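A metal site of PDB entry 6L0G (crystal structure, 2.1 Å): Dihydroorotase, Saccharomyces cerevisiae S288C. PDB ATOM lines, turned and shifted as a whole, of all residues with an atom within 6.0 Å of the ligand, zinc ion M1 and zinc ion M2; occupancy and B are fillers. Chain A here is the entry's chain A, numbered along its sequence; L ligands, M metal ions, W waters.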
ATOM      1  N   HIS A  14       6.139  33.334  15.828  1.00  0.00           N
ATOM      2  CA  HIS A  14       5.983  32.322  16.898  1.00  0.00           C
ATOM      3  C   HIS A  14       4.697  32.628  17.668  1.00  0.00           C
ATOM      4  O   HIS A  14       4.719  33.402  18.628  1.00  0.00           O
ATOM      5  CB  HIS A  14       7.212  32.325  17.805  1.00  0.00           C
ATOM      6  CG  HIS A  14       7.351  31.076  18.651  1.00  0.00           C
ATOM      7  ND1 HIS A  14       8.539  30.395  18.778  1.00  0.00           N
ATOM      8  CD2 HIS A  14       6.460  30.434  19.443  1.00  0.00           C
ATOM      9  CE1 HIS A  14       8.364  29.366  19.593  1.00  0.00           C
ATOM     10  NE2 HIS A  14       7.125  29.373  20.016  1.00  0.00           N
ATOM     11  N   HIS A  16       0.942  31.197  19.472  1.00  0.00           N
ATOM     12  CA  HIS A  16       0.015  30.185  19.993  1.00  0.00           C
ATOM     13  C   HIS A  16      -1.397  30.757  20.079  1.00  0.00           C
ATOM     14  O   HIS A  16      -1.610  31.780  20.745  1.00  0.00           O
ATOM     15  CB  HIS A  16       0.460  29.695  21.374  1.00  0.00           C
ATOM     16  CG  HIS A  16       1.804  29.008  21.376  1.00  0.00           C
ATOM     17  ND1 HIS A  16       1.940  27.651  21.195  1.00  0.00           N
ATOM     18  CD2 HIS A  16       3.049  29.503  21.521  1.00  0.00           C
ATOM     19  CE1 HIS A  16       3.227  27.330  21.230  1.00  0.00           C
ATOM     20  NE2 HIS A  16       3.920  28.441  21.424  1.00  0.00           N
ATOM     21  N   ARG A  18      -4.240  28.299  20.449  1.00  0.00           N
ATOM     22  CA  ARG A  18      -5.018  27.252  21.130  1.00  0.00           C
ATOM     23  C   ARG A  18      -6.196  26.798  20.249  1.00  0.00           C
ATOM     24  O   ARG A  18      -6.068  26.737  19.014  1.00  0.00           O
ATOM     25  CB  ARG A  18      -5.438  27.736  22.514  1.00  0.00           C
ATOM     26  CG  ARG A  18      -4.336  28.511  23.311  1.00  0.00           C
ATOM     27  CD  ARG A  18      -3.058  27.678  23.576  1.00  0.00           C
ATOM     28  NE  ARG A  18      -2.238  28.301  24.606  1.00  0.00           N
ATOM     29  CZ  ARG A  18      -0.961  28.034  24.857  1.00  0.00           C
ATOM     30  NH1 ARG A  18      -0.304  27.124  24.135  1.00  0.00           N
ATOM     31  NH2 ARG A  18      -0.328  28.692  25.835  1.00  0.00           N
ATOM     32  N   MET A  41       2.011  27.847  15.893  1.00  0.00           N
ATOM     33  CA  MET A  41       2.626  26.652  16.467  1.00  0.00           C
ATOM     34  C   MET A  41       1.609  25.519  16.634  1.00  0.00           C
ATOM     35  O   MET A  41       0.412  25.768  16.704  1.00  0.00           O
ATOM     36  CB  MET A  41       3.265  27.015  17.804  1.00  0.00           C
ATOM     37  CG  MET A  41       4.501  27.941  17.626  1.00  0.00           C
ATOM     38  SD  MET A  41       5.728  27.093  16.624  1.00  0.00           S
ATOM     39  CE  MET A  41       7.044  28.268  16.398  1.00  0.00           C
ATOM     40  N   ASN A  43       1.337  22.830  19.054  1.00  0.00           N
ATOM     41  CA  ASN A  43       1.300  22.033  20.285  1.00  0.00           C
ATOM     42  C   ASN A  43      -0.115  22.060  20.904  1.00  0.00           C
ATOM     43  O   ASN A  43      -0.331  22.470  22.040  1.00  0.00           O
ATOM     44  CB  ASN A  43       2.366  22.507  21.269  1.00  0.00           C
ATOM     45  CG  ASN A  43       2.153  23.941  21.739  1.00  0.00           C
ATOM     46  OD1 ASN A  43       1.540  24.743  21.044  1.00  0.00           O
ATOM     47  ND2 ASN A  43       2.647  24.261  22.936  1.00  0.00           N
ATOM     48  N   KCX A  98       7.836  22.025  13.957  1.00  0.00           N
ATOM     49  CA  KCX A  98       8.299  22.534  15.241  1.00  0.00           C
ATOM     50  CB  KCX A  98       7.221  23.374  15.935  1.00  0.00           C
ATOM     51  CG  KCX A  98       7.561  23.728  17.382  1.00  0.00           C
ATOM     52  CD  KCX A  98       8.738  24.705  17.426  1.00  0.00           C
ATOM     53  CE  KCX A  98       8.951  25.274  18.822  1.00  0.00           C
ATOM     54  NZ  KCX A  98       7.646  25.782  19.290  1.00  0.00           N
ATOM     55  C   KCX A  98       8.705  21.404  16.165  1.00  0.00           C
ATOM     56  O   KCX A  98       7.924  20.484  16.401  1.00  0.00           O
ATOM     57  CX  KCX A  98       7.526  26.379  20.470  1.00  0.00           C
ATOM     58  OQ1 KCX A  98       6.408  26.768  20.834  1.00  0.00           O
ATOM     59  OQ2 KCX A  98       8.504  26.508  21.223  1.00  0.00           O
ATOM     60  N   TYR A 100       9.533  20.127  19.894  1.00  0.00           N
ATOM     61  CA  TYR A 100       9.472  20.264  21.341  1.00  0.00           C
ATOM     62  C   TYR A 100      10.239  19.118  21.991  1.00  0.00           C
ATOM     63  O   TYR A 100       9.902  17.963  21.742  1.00  0.00           O
ATOM     64  CB  TYR A 100       8.007  20.255  21.849  1.00  0.00           C
ATOM     65  CG  TYR A 100       7.169  21.428  21.369  1.00  0.00           C
ATOM     66  CD1 TYR A 100       7.221  22.636  22.018  1.00  0.00           C
ATOM     67  CD2 TYR A 100       6.347  21.298  20.244  1.00  0.00           C
ATOM     68  CE1 TYR A 100       6.453  23.701  21.571  1.00  0.00           C
ATOM     69  CE2 TYR A 100       5.590  22.354  19.799  1.00  0.00           C
ATOM     70  CZ  TYR A 100       5.638  23.560  20.462  1.00  0.00           C
ATOM     71  OH  TYR A 100       4.885  24.617  20.004  1.00  0.00           O
ATOM     72  N   VAL A 104       9.574  19.661  28.388  1.00  0.00           N
ATOM     73  CA  VAL A 104      10.174  20.942  28.775  1.00  0.00           C
ATOM     74  C   VAL A 104       9.167  22.092  28.785  1.00  0.00           C
ATOM     75  O   VAL A 104       9.466  23.132  29.401  1.00  0.00           O
ATOM     76  CB  VAL A 104      11.379  21.331  27.896  1.00  0.00           C
ATOM     77  CG1 VAL A 104      12.477  20.261  27.972  1.00  0.00           C
ATOM     78  CG2 VAL A 104      10.965  21.570  26.447  1.00  0.00           C
ATOM     79  N   THR A 105       7.994  21.939  28.178  1.00  0.00           N
ATOM     80  CA  THR A 105       7.059  23.065  28.139  1.00  0.00           C
ATOM     81  C   THR A 105       5.639  22.578  27.852  1.00  0.00           C
ATOM     82  O   THR A 105       5.342  21.376  27.907  1.00  0.00           O
ATOM     83  CB  THR A 105       7.527  24.097  27.107  1.00  0.00           C
ATOM     84  OG1 THR A 105       6.793  25.302  27.277  1.00  0.00           O
ATOM     85  CG2 THR A 105       7.354  23.584  25.694  1.00  0.00           C
ATOM     86  N   THR A 106       4.740  23.537  27.595  1.00  0.00           N
ATOM     87  CA  THR A 106       3.319  23.258  27.424  1.00  0.00           C
ATOM     88  C   THR A 106       3.076  22.266  26.279  1.00  0.00           C
ATOM     89  O   THR A 106       3.527  22.482  25.150  1.00  0.00           O
ATOM     90  CB  THR A 106       2.557  24.555  27.120  1.00  0.00           C
ATOM     91  OG1 THR A 106       2.751  25.508  28.191  1.00  0.00           O
ATOM     92  CG2 THR A 106       1.084  24.284  26.964  1.00  0.00           C
ATOM     93  N   ASN A 107       2.332  21.195  26.585  1.00  0.00           N
ATOM     94  CA  ASN A 107       1.932  20.182  25.598  1.00  0.00           C
ATOM     95  C   ASN A 107       3.134  19.617  24.843  1.00  0.00           C
ATOM     96  O   ASN A 107       3.117  19.441  23.614  1.00  0.00           O
ATOM     97  CB  ASN A 107       0.890  20.748  24.637  1.00  0.00           C
ATOM     98  CG  ASN A 107      -0.458  20.976  25.324  1.00  0.00           C
ATOM     99  OD1 ASN A 107      -0.727  20.397  26.368  1.00  0.00           O
ATOM    100  ND2 ASN A 107      -1.300  21.837  24.732  1.00  0.00           N
ATOM    101  N   HIS A 137      12.499  24.370  19.793  1.00  0.00           N
ATOM    102  CA  HIS A 137      12.503  24.843  21.170  1.00  0.00           C
ATOM    103  C   HIS A 137      13.779  24.269  21.760  1.00  0.00           C
ATOM    104  O   HIS A 137      13.838  23.117  22.186  1.00  0.00           O
ATOM    105  CB  HIS A 137      11.260  24.398  21.931  1.00  0.00           C
ATOM    106  CG  HIS A 137      11.237  24.872  23.361  1.00  0.00           C
ATOM    107  ND1 HIS A 137      10.157  25.560  23.903  1.00  0.00           N
ATOM    108  CD2 HIS A 137      12.154  24.768  24.350  1.00  0.00           C
ATOM    109  CE1 HIS A 137      10.415  25.838  25.170  1.00  0.00           C
ATOM    110  NE2 HIS A 137      11.616  25.359  25.469  1.00  0.00           N
ATOM    111  N   GLU A 179      14.216  29.017  18.304  1.00  0.00           N
ATOM    112  CA  GLU A 179      13.115  29.857  18.744  1.00  0.00           C
ATOM    113  C   GLU A 179      13.422  30.485  20.105  1.00  0.00           C
ATOM    114  O   GLU A 179      14.202  29.952  20.901  1.00  0.00           O
ATOM    115  CB  GLU A 179      11.817  29.044  18.862  1.00  0.00           C
ATOM    116  CG  GLU A 179      11.298  28.473  17.543  1.00  0.00           C
ATOM    117  CD  GLU A 179      10.860  29.544  16.563  1.00  0.00           C
ATOM    118  OE1 GLU A 179      10.481  30.649  17.019  1.00  0.00           O
ATOM    119  OE2 GLU A 179      10.894  29.275  15.333  1.00  0.00           O
ATOM    120  N   HIS A 180      12.795  31.642  20.352  1.00  0.00           N
ATOM    121  CA  HIS A 180      12.842  32.384  21.606  1.00  0.00           C
ATOM    122  C   HIS A 180      14.153  32.211  22.360  1.00  0.00           C
ATOM    123  O   HIS A 180      14.195  31.546  23.404  1.00  0.00           O
ATOM    124  CB  HIS A 180      11.636  32.041  22.507  1.00  0.00           C
ATOM    125  CG  HIS A 180      11.275  30.580  22.568  1.00  0.00           C
ATOM    126  ND1 HIS A 180      12.224  29.584  22.684  1.00  0.00           N
ATOM    127  CD2 HIS A 180      10.085  29.954  22.606  1.00  0.00           C
ATOM    128  CE1 HIS A 180      11.628  28.410  22.757  1.00  0.00           C
ATOM    129  NE2 HIS A 180      10.330  28.603  22.697  1.00  0.00           N
ATOM    130  N   CYS A 229       7.740  31.551  31.948  1.00  0.00           N
ATOM    131  CA  CYS A 229       7.607  30.970  30.626  1.00  0.00           C
ATOM    132  C   CYS A 229       8.804  30.064  30.399  1.00  0.00           C
ATOM    133  O   CYS A 229       9.765  30.090  31.175  1.00  0.00           O
ATOM    134  CB  CYS A 229       7.508  32.078  29.553  1.00  0.00           C
ATOM    135  SG  CYS A 229       9.056  33.014  29.367  1.00  0.00           S
ATOM    136  N   LYS A 230       8.762  29.282  29.297  1.00  0.00           N
ATOM    137  CA  LYS A 230       9.936  28.548  28.851  1.00  0.00           C
ATOM    138  C   LYS A 230      10.411  29.076  27.494  1.00  0.00           C
ATOM    139  O   LYS A 230       9.578  29.405  26.649  1.00  0.00           O
ATOM    140  CB  LYS A 230       9.632  27.055  28.745  1.00  0.00           C
ATOM    141  CG  LYS A 230       9.289  26.368  30.071  1.00  0.00           C
ATOM    142  CD  LYS A 230      10.384  26.601  31.101  1.00  0.00           C
ATOM    143  CE  LYS A 230      11.526  25.638  30.855  1.00  0.00           C
ATOM    144  NZ  LYS A 230      11.162  24.243  31.322  1.00  0.00           N
ATOM    145  N   PRO A 231      11.735  29.194  27.259  1.00  0.00           N
ATOM    146  CA  PRO A 231      12.794  29.122  28.289  1.00  0.00           C
ATOM    147  C   PRO A 231      12.659  30.269  29.291  1.00  0.00           C
ATOM    148  O   PRO A 231      12.133  31.337  28.926  1.00  0.00           O
ATOM    149  CB  PRO A 231      14.104  29.230  27.473  1.00  0.00           C
ATOM    150  CG  PRO A 231      13.674  29.147  25.989  1.00  0.00           C
ATOM    151  CD  PRO A 231      12.280  29.700  25.988  1.00  0.00           C
ATOM    152  N   ASP A 258       6.189  34.267  20.808  1.00  0.00           N
ATOM    153  CA  ASP A 258       5.797  33.155  21.656  1.00  0.00           C
ATOM    154  C   ASP A 258       4.670  33.560  22.602  1.00  0.00           C
ATOM    155  O   ASP A 258       4.637  33.183  23.774  1.00  0.00           O
ATOM    156  CB  ASP A 258       6.990  32.602  22.456  1.00  0.00           C
ATOM    157  CG  ASP A 258       6.674  31.264  23.155  1.00  0.00           C
ATOM    158  OD1 ASP A 258       5.724  30.577  22.741  1.00  0.00           O
ATOM    159  OD2 ASP A 258       7.381  30.925  24.141  1.00  0.00           O
ATOM    160  N   SER A 259       3.733  34.359  22.084  1.00  0.00           N
ATOM    161  CA  SER A 259       2.543  34.660  22.875  1.00  0.00           C
ATOM    162  C   SER A 259       1.794  33.356  23.142  1.00  0.00           C
ATOM    163  O   SER A 259       1.473  32.621  22.209  1.00  0.00           O
ATOM    164  CB  SER A 259       1.655  35.662  22.157  1.00  0.00           C
ATOM    165  OG  SER A 259       0.442  35.854  22.865  1.00  0.00           O
ATOM    166  N   ALA A 260       1.587  33.060  24.423  1.00  0.00           N
ATOM    167  CA  ALA A 260       1.107  31.747  24.882  1.00  0.00           C
ATOM    168  C   ALA A 260      -0.046  31.931  25.861  1.00  0.00           C
ATOM    169  O   ALA A 260       0.172  32.032  27.080  1.00  0.00           O
ATOM    170  CB  ALA A 260       2.239  30.959  25.521  1.00  0.00           C
ATOM    171  N   PRO A 261      -1.290  31.972  25.375  1.00  0.00           N
ATOM    172  CA  PRO A 261      -2.419  32.265  26.266  1.00  0.00           C
ATOM    173  C   PRO A 261      -2.733  31.109  27.205  1.00  0.00           C
ATOM    174  O   PRO A 261      -2.785  29.949  26.803  1.00  0.00           O
ATOM    175  CB  PRO A 261      -3.585  32.524  25.315  1.00  0.00           C
ATOM    176  CG  PRO A 261      -3.191  31.960  24.014  1.00  0.00           C
ATOM    177  CD  PRO A 261      -1.713  31.771  23.972  1.00  0.00           C
ATOM    178  N   HIS A 262      -2.967  31.450  28.482  1.00  0.00           N
ATOM    179  CA  HIS A 262      -3.455  30.533  29.503  1.00  0.00           C
ATOM    180  C   HIS A 262      -4.555  31.215  30.300  1.00  0.00           C
ATOM    181  O   HIS A 262      -4.428  32.407  30.641  1.00  0.00           O
ATOM    182  CB  HIS A 262      -2.330  30.106  30.452  1.00  0.00           C
ATOM    183  CG  HIS A 262      -1.274  29.269  29.796  1.00  0.00           C
ATOM    184  ND1 HIS A 262      -1.496  27.948  29.466  1.00  0.00           N
ATOM    185  CD2 HIS A 262      -0.017  29.554  29.410  1.00  0.00           C
ATOM    186  CE1 HIS A 262      -0.406  27.452  28.890  1.00  0.00           C
ATOM    187  NE2 HIS A 262       0.503  28.406  28.848  1.00  0.00           N
ATOM    188  N   ALA A 275       3.495  27.368  31.818  1.00  0.00           N
ATOM    189  CA  ALA A 275       4.511  28.251  31.282  1.00  0.00           C
ATOM    190  C   ALA A 275       3.951  29.042  30.107  1.00  0.00           C
ATOM    191  O   ALA A 275       3.316  28.473  29.209  1.00  0.00           O
ATOM    192  CB  ALA A 275       5.728  27.445  30.830  1.00  0.00           C
ATOM    193  N   GLY A 276       4.222  30.330  30.088  1.00  0.00           N
ATOM    194  CA  GLY A 276       3.823  31.141  28.951  1.00  0.00           C
ATOM    195  C   GLY A 276       3.394  32.547  29.283  1.00  0.00           C
ATOM    196  O   GLY A 276       2.720  32.793  30.298  1.00  0.00           O
ATOM    197  N   VAL A 277       3.790  33.486  28.424  1.00  0.00           N
ATOM    198  CA  VAL A 277       3.464  34.899  28.572  1.00  0.00           C
ATOM    199  C   VAL A 277       2.565  35.274  27.407  1.00  0.00           C
ATOM    200  O   VAL A 277       2.883  34.936  26.254  1.00  0.00           O
ATOM    201  CB  VAL A 277       4.745  35.763  28.592  1.00  0.00           C
ATOM    202  CG1 VAL A 277       4.405  37.254  28.606  1.00  0.00           C
ATOM    203  CG2 VAL A 277       5.617  35.408  29.796  1.00  0.00           C
HETATM  204  C1  LIG L   1       6.437  27.352  24.892  1.00  0.00           C
HETATM  205  O1  LIG L   1       6.648  27.977  23.814  1.00  0.00           O
HETATM  206  O2  LIG L   1       7.432  26.873  25.463  1.00  0.00           O
HETATM  207  C2  LIG L   1       5.029  27.177  25.503  1.00  0.00           C
HETATM  208  O3  LIG L   1       4.796  27.847  26.720  1.00  0.00           O
HETATM  209  C3  LIG L   1       4.061  27.827  24.585  1.00  0.00           C
HETATM  210  C4  LIG L   1       2.744  27.300  25.094  1.00  0.00           C
HETATM  211  O4  LIG L   1       2.342  27.515  26.284  1.00  0.00           O
HETATM  212  O5  LIG L   1       2.092  26.664  24.233  1.00  0.00           O
HETATM  213 ZN    ZN M   1       6.006  28.721  21.717  1.00  0.00          ZN
HETATM  214 ZN    ZN M   2       8.887  27.072  23.030  1.00  0.00          ZN
HETATM  215  O   HOH W   1       6.690  29.886  27.069  1.00  0.00           O
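ND2 of Asn 43 lies within hydrogen-bond range of O5 of the ligand (2.8 Å).
The guanidinium group (NH1) of Arg 18 is in salt-bridge range of an oxygen (O5) of the ligand (2.4 Å).
NE2 of His 262 lies within hydrogen-bond range of O4 of the ligand (3.3 Å).
The side-chain hydroxyl (OG1) of Thr 105 lies within hydrogen-bond range of an oxygen (O2) of the ligand, 2.5 Å away.
The backbone carbonyl oxygen (O) of Ala 275 sits at hydrogen-bond distance from an oxygen (O3) of the ligand, at 3.0 Å.
The side-chain hydroxyl of Thr 106 lies within hydrogen-bond range of an oxygen (O4) of the ligand (2.8 Å).
The backbone carbonyl oxygen (O) of Ala 275 lies within hydrogen-bond range of a ring nitrogen (NE2) of His 262 (2.8 Å).
The side-chain hydroxyl (OH) of Tyr 100 sits at hydrogen-bond distance from NZ of KCX 98, 3.1 Å away.
The backbone NH (N) of Ala 260 is in hydrogen-bond range of the backbone carbonyl oxygen (O) of Val 277 (2.9 Å).
A ring nitrogen (ND1) of His 14 is in hydrogen-bond range of the side-chain carboxylate of Glu 179, 2.6 Å away.
NH2 of Arg 18 lies within hydrogen-bond range of NE2 of His 262 (3.1 Å).
O of Ala 275 lies within hydrogen-bond range of OG1 of Thr 106 (3.2 Å).
The backbone carbonyl oxygen (O) of Asn 43 lies within hydrogen-bond range of the side-chain amide nitrogen (ND2) of Asn 107 (2.9 Å).
The backbone carbonyl oxygen of Ser 259 lies within hydrogen-bond range of the backbone NH of His 16.
Residues that only touch the ligand: Lys 230 and Ala 260.
Hydrophobic or aromatic side chains within 4 Å of the ligand: His 16, His 137, Ala 260 and His 262.
Of the 25 residues printed, 13 come within 4 Å of the ligand.
The nearest printed residue that does not touch the ligand is His 14 (4.1 Å).
Within 4 Å of zinc ion M1: His 14, His 16, KCX 98 and Asp 258.
The nearest printed residue that does not touch zinc ion M1 is His 180 (4.4 Å).
Of the 25 residues printed, 3 come within 4 Å of zinc ion M2.
The nearest printed residue that does not touch zinc ion M2 is His 14 (4.2 Å).
NE2 of His 16 is bound to zinc ion M1 (2.1 Å).
NE2 of His 14 binds zinc ion M1 (2.1 Å).
OD1 of Asp 258 binds zinc ion M1 (2.1 Å).
Zinc ion M1 is bound by OQ1 of KCX 98, at 2.2 Å.
Zinc ion M1 is bound by O1 of the ligand (2.3 Å).
Zinc ion M1 has five donor atoms within binding distance.
Zinc ion M2 is bound by OQ2 of KCX 98.
A ring nitrogen (NE2) of His 180 is bound to zinc ion M2 (2.1 Å).
Zinc ion M2 is bound by ND1 of His 137 (2.2 Å).
O1 of the ligand is bound to zinc ion M2 (2.5 Å).
Zinc ion M2 has four donor atoms within binding distance.
Slightly farther from zinc ion M2 lies O2 of the ligand (2.8 Å).
Water W1 lies within hydrogen-bond range of O3 of the ligand, O of Lys 230 and OD2 of Asp 258.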
